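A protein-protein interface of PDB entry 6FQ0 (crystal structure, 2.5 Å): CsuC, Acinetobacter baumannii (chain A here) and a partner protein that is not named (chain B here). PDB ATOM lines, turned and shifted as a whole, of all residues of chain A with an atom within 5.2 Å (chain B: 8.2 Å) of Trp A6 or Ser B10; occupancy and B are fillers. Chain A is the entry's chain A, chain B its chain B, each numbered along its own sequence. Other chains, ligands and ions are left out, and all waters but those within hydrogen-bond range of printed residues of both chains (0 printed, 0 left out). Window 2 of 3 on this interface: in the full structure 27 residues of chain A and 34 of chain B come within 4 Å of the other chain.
Of chain A, only Trp A6 (3.1 Å) comes within 4 Å of Ser B10.
Pro A7 touches one residue of chain B.
Of the printed residues of chain B, Ile A5 touches Gly B12 and Cys B13.
Of the printed residues of chain B, Ile A8 touches Thr B11 and Cys B13.
Asp B61 touches none of the printed residues of chain A.
His B9 touches none of the printed residues of chain A.
The nearest residue of chain B that does not touch Trp A6 is Asp B61 (4.7 Å).
The nearest residue of chain A that does not touch Ser B10 is Pro A7 (4.2 Å).
The backbone carbonyl oxygen of Trp A6 lies within hydrogen-bond range of the backbone NH of Trp A22, at 2.7 Å.
The backbone NH of Gly B12 lies within hydrogen-bond range of the side-chain carboxylate of Asp B61 (2.6 Å).
The side-chain sulfur (SG) of Cys B13 forms a disulfide with the side-chain sulfur (SG) of Cys B60, at 2.0 Å.
Among the printed residues, merely in contact across the chains: Ile A5 with Gly B12 (3.3 Å), Leu A4 with Cys B13 (3.6 Å), Trp A6 with Gly B12 (3.6 Å), Pro A7 with Thr B11 (3.7 Å), Leu A4 with Thr B14 (3.8 Å), Ile A8 with Cys B13 (3.8 Å) and Trp A6 with Thr B11 (3.9 Å).
The backbone NH (N) of Ile A5 lies within hydrogen-bond range of the backbone carbonyl oxygen (O) of Cys B13 (3.0 Å).
The indole nitrogen of Trp A6 sits at hydrogen-bond distance from the backbone carbonyl oxygen of Ser B10.
The backbone NH (N) of Ile A8 is in hydrogen-bond range of the backbone carbonyl oxygen (O) of Thr B11 (2.9 Å).
Among the printed residues, 10 pairs touch across the chains.
Among the printed residues, no Asp or Glu carboxylate lies within 4 Å of a Lys or Arg side-chain nitrogen of the other chain.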
ATOM      1  N   LEU A   4      13.876  38.560  -5.735  1.00  0.00           N
ATOM      2  CA  LEU A   4      13.673  37.170  -6.118  1.00  0.00           C
ATOM      3  C   LEU A   4      13.262  36.388  -4.878  1.00  0.00           C
ATOM      4  O   LEU A   4      13.970  36.407  -3.865  1.00  0.00           O
ATOM      5  CB  LEU A   4      14.939  36.575  -6.736  1.00  0.00           C
ATOM      6  CG  LEU A   4      14.943  35.069  -7.019  1.00  0.00           C
ATOM      7  CD1 LEU A   4      13.710  34.654  -7.814  1.00  0.00           C
ATOM      8  CD2 LEU A   4      16.217  34.666  -7.747  1.00  0.00           C
ATOM      9  N   ILE A   5      12.122  35.708  -4.958  1.00  0.00           N
ATOM     10  CA  ILE A   5      11.556  34.973  -3.833  1.00  0.00           C
ATOM     11  C   ILE A   5      11.527  33.497  -4.200  1.00  0.00           C
ATOM     12  O   ILE A   5      10.885  33.107  -5.183  1.00  0.00           O
ATOM     13  CB  ILE A   5      10.150  35.477  -3.473  1.00  0.00           C
ATOM     14  CG1 ILE A   5      10.198  36.954  -3.079  1.00  0.00           C
ATOM     15  CG2 ILE A   5       9.559  34.648  -2.343  1.00  0.00           C
ATOM     16  CD1 ILE A   5       8.834  37.596  -2.953  1.00  0.00           C
ATOM     17  N   TRP A   6      12.228  32.677  -3.414  1.00  0.00           N
ATOM     18  CA  TRP A   6      12.308  31.256  -3.675  1.00  0.00           C
ATOM     19  C   TRP A   6      12.386  30.515  -2.347  1.00  0.00           C
ATOM     20  O   TRP A   6      13.231  30.866  -1.507  1.00  0.00           O
ATOM     21  CB  TRP A   6      13.520  30.908  -4.541  1.00  0.00           C
ATOM     22  CG  TRP A   6      13.587  29.463  -4.924  1.00  0.00           C
ATOM     23  CD1 TRP A   6      13.086  28.895  -6.058  1.00  0.00           C
ATOM     24  CD2 TRP A   6      14.188  28.399  -4.175  1.00  0.00           C
ATOM     25  NE1 TRP A   6      13.337  27.545  -6.062  1.00  0.00           N
ATOM     26  CE2 TRP A   6      14.012  27.215  -4.917  1.00  0.00           C
ATOM     27  CE3 TRP A   6      14.857  28.334  -2.948  1.00  0.00           C
ATOM     28  CZ2 TRP A   6      14.481  25.980  -4.474  1.00  0.00           C
ATOM     29  CZ3 TRP A   6      15.321  27.105  -2.510  1.00  0.00           C
ATOM     30  CH2 TRP A   6      15.131  25.946  -3.271  1.00  0.00           C
ATOM     31  N   PRO A   7      11.533  29.505  -2.121  1.00  0.00           N
ATOM     32  CA  PRO A   7      10.469  29.113  -3.049  1.00  0.00           C
ATOM     33  C   PRO A   7       9.202  29.946  -2.873  1.00  0.00           C
ATOM     34  O   PRO A   7       8.992  30.542  -1.817  1.00  0.00           O
ATOM     35  CB  PRO A   7      10.216  27.655  -2.678  1.00  0.00           C
ATOM     36  CG  PRO A   7      10.474  27.621  -1.208  1.00  0.00           C
ATOM     37  CD  PRO A   7      11.606  28.598  -0.961  1.00  0.00           C
ATOM     38  N   ILE A   8       8.365  29.987  -3.910  1.00  0.00           N
ATOM     39  CA  ILE A   8       7.118  30.736  -3.817  1.00  0.00           C
ATOM     40  C   ILE A   8       6.028  29.943  -3.106  1.00  0.00           C
ATOM     41  O   ILE A   8       5.022  30.528  -2.684  1.00  0.00           O
ATOM     42  CB  ILE A   8       6.662  31.181  -5.219  1.00  0.00           C
ATOM     43  CG1 ILE A   8       6.015  32.564  -5.153  1.00  0.00           C
ATOM     44  CG2 ILE A   8       5.717  30.163  -5.837  1.00  0.00           C
ATOM     45  CD1 ILE A   8       7.010  33.692  -5.005  1.00  0.00           C
ATOM     46  N   ALA A  20      12.994  27.199   4.946  1.00  0.00           N
ATOM     47  CA  ALA A  20      13.672  28.427   4.561  1.00  0.00           C
ATOM     48  C   ALA A  20      13.054  29.011   3.300  1.00  0.00           C
ATOM     49  O   ALA A  20      12.739  28.282   2.353  1.00  0.00           O
ATOM     50  CB  ALA A  20      15.167  28.189   4.339  1.00  0.00           C
ATOM     51  N   VAL A  21      12.874  30.330   3.302  1.00  0.00           N
ATOM     52  CA  VAL A  21      12.511  31.098   2.118  1.00  0.00           C
ATOM     53  C   VAL A  21      13.623  32.106   1.871  1.00  0.00           C
ATOM     54  O   VAL A  21      14.077  32.773   2.807  1.00  0.00           O
ATOM     55  CB  VAL A  21      11.154  31.808   2.287  1.00  0.00           C
ATOM     56  CG1 VAL A  21      10.829  32.637   1.051  1.00  0.00           C
ATOM     57  CG2 VAL A  21      10.054  30.795   2.562  1.00  0.00           C
ATOM     58  N   TRP A  22      14.063  32.217   0.624  1.00  0.00           N
ATOM     59  CA  TRP A  22      15.183  33.083   0.283  1.00  0.00           C
ATOM     60  C   TRP A  22      14.692  34.367  -0.371  1.00  0.00           C
ATOM     61  O   TRP A  22      13.914  34.328  -1.330  1.00  0.00           O
ATOM     62  CB  TRP A  22      16.170  32.360  -0.631  1.00  0.00           C
ATOM     63  CG  TRP A  22      17.124  31.489   0.126  1.00  0.00           C
ATOM     64  CD1 TRP A  22      18.349  31.845   0.610  1.00  0.00           C
ATOM     65  CD2 TRP A  22      16.927  30.119   0.502  1.00  0.00           C
ATOM     66  NE1 TRP A  22      18.930  30.782   1.257  1.00  0.00           N
ATOM     67  CE2 TRP A  22      18.078  29.711   1.205  1.00  0.00           C
ATOM     68  CE3 TRP A  22      15.892  29.199   0.309  1.00  0.00           C
ATOM     69  CZ2 TRP A  22      18.223  28.422   1.716  1.00  0.00           C
ATOM     70  CZ3 TRP A  22      16.038  27.919   0.818  1.00  0.00           C
ATOM     71  CH2 TRP A  22      17.195  27.543   1.512  1.00  0.00           C
ATOM     72  N   HIS B   8      10.641  17.252  -8.764  1.00  0.00           N
ATOM     73  CA  HIS B   8       9.887  18.431  -8.355  1.00  0.00           C
ATOM     74  C   HIS B   8      10.689  19.710  -8.569  1.00  0.00           C
ATOM     75  O   HIS B   8      11.816  19.838  -8.089  1.00  0.00           O
ATOM     76  CB  HIS B   8       9.470  18.320  -6.887  1.00  0.00           C
ATOM     77  CG  HIS B   8       8.852  19.568  -6.337  1.00  0.00           C
ATOM     78  ND1 HIS B   8       7.767  20.183  -6.923  1.00  0.00           N
ATOM     79  CD2 HIS B   8       9.169  20.317  -5.254  1.00  0.00           C
ATOM     80  CE1 HIS B   8       7.443  21.258  -6.225  1.00  0.00           C
ATOM     81  NE2 HIS B   8       8.279  21.361  -5.207  1.00  0.00           N
ATOM     82  N   HIS B   9      10.100  20.655  -9.294  1.00  0.00           N
ATOM     83  CA  HIS B   9      10.714  21.952  -9.542  1.00  0.00           C
ATOM     84  C   HIS B   9      10.044  22.994  -8.654  1.00  0.00           C
ATOM     85  O   HIS B   9       8.833  23.216  -8.758  1.00  0.00           O
ATOM     86  CB  HIS B   9      10.591  22.346 -11.014  1.00  0.00           C
ATOM     87  CG  HIS B   9      10.899  23.787 -11.280  1.00  0.00           C
ATOM     88  ND1 HIS B   9      12.183  24.287 -11.281  1.00  0.00           N
ATOM     89  CD2 HIS B   9      10.088  24.838 -11.547  1.00  0.00           C
ATOM     90  CE1 HIS B   9      12.150  25.582 -11.542  1.00  0.00           C
ATOM     91  NE2 HIS B   9      10.890  25.941 -11.706  1.00  0.00           N
ATOM     92  N   SER B  10      10.831  23.628  -7.789  1.00  0.00           N
ATOM     93  CA  SER B  10      10.317  24.685  -6.927  1.00  0.00           C
ATOM     94  C   SER B  10      10.302  25.998  -7.699  1.00  0.00           C
ATOM     95  O   SER B  10      11.343  26.447  -8.192  1.00  0.00           O
ATOM     96  CB  SER B  10      11.168  24.811  -5.666  1.00  0.00           C
ATOM     97  OG  SER B  10      10.856  23.789  -4.735  1.00  0.00           O
ATOM     98  N   THR B  11       9.127  26.613  -7.798  1.00  0.00           N
ATOM     99  CA  THR B  11       8.993  27.865  -8.528  1.00  0.00           C
ATOM    100  C   THR B  11       9.548  29.027  -7.714  1.00  0.00           C
ATOM    101  O   THR B  11       9.180  29.217  -6.551  1.00  0.00           O
ATOM    102  CB  THR B  11       7.527  28.124  -8.876  1.00  0.00           C
ATOM    103  OG1 THR B  11       7.017  27.025  -9.641  1.00  0.00           O
ATOM    104  CG2 THR B  11       7.380  29.412  -9.682  1.00  0.00           C
ATOM    105  N   GLY B  12      10.430  29.805  -8.335  1.00  0.00           N
ATOM    106  CA  GLY B  12      10.799  31.099  -7.803  1.00  0.00           C
ATOM    107  C   GLY B  12      10.223  32.193  -8.674  1.00  0.00           C
ATOM    108  O   GLY B  12       9.940  31.958  -9.852  1.00  0.00           O
ATOM    109  N   CYS B  13      10.041  33.391  -8.124  1.00  0.00           N
ATOM    110  CA  CYS B  13       9.464  34.488  -8.884  1.00  0.00           C
ATOM    111  C   CYS B  13      10.195  35.780  -8.561  1.00  0.00           C
ATOM    112  O   CYS B  13      10.470  36.075  -7.394  1.00  0.00           O
ATOM    113  CB  CYS B  13       7.967  34.659  -8.591  1.00  0.00           C
ATOM    114  SG  CYS B  13       6.913  33.256  -9.035  1.00  0.00           S
ATOM    115  N   THR B  14      10.502  36.544  -9.604  1.00  0.00           N
ATOM    116  CA  THR B  14      11.075  37.873  -9.458  1.00  0.00           C
ATOM    117  C   THR B  14       9.956  38.904  -9.466  1.00  0.00           C
ATOM    118  O   THR B  14       9.134  38.932 -10.388  1.00  0.00           O
ATOM    119  CB  THR B  14      12.072  38.168 -10.578  1.00  0.00           C
ATOM    120  OG1 THR B  14      13.170  37.251 -10.494  1.00  0.00           O
ATOM    121  CG2 THR B  14      12.600  39.591 -10.457  1.00  0.00           C
ATOM    122  N   CYS B  60       8.358  34.377 -13.183  1.00  0.00           N
ATOM    123  CA  CYS B  60       8.577  33.134 -12.460  1.00  0.00           C
ATOM    124  C   CYS B  60       9.334  32.137 -13.331  1.00  0.00           C
ATOM    125  O   CYS B  60       9.162  32.096 -14.553  1.00  0.00           O
ATOM    126  CB  CYS B  60       7.249  32.532 -11.990  1.00  0.00           C
ATOM    127  SG  CYS B  60       6.275  33.636 -10.929  1.00  0.00           S
ATOM    128  N   ASP B  61      10.176  31.332 -12.680  1.00  0.00           N
ATOM    129  CA  ASP B  61      11.165  30.497 -13.354  1.00  0.00           C
ATOM    130  C   ASP B  61      10.621  29.165 -13.858  1.00  0.00           C
ATOM    131  O   ASP B  61      11.364  28.431 -14.519  1.00  0.00           O
ATOM    132  CB  ASP B  61      12.349  30.234 -12.416  1.00  0.00           C
ATOM    133  CG  ASP B  61      11.986  29.317 -11.255  1.00  0.00           C
ATOM    134  OD1 ASP B  61      10.793  29.254 -10.886  1.00  0.00           O
ATOM    135  OD2 ASP B  61      12.895  28.659 -10.706  1.00  0.00           O
ATOM    136  N   GLY B  62       9.369  28.826 -13.581  1.00  0.00           N
ATOM    137  CA  GLY B  62       8.856  27.517 -13.926  1.00  0.00           C
ATOM    138  C   GLY B  62       8.548  27.363 -15.402  1.00  0.00           C
ATOM    139  O   GLY B  62       8.960  28.161 -16.246  1.00  0.00           O
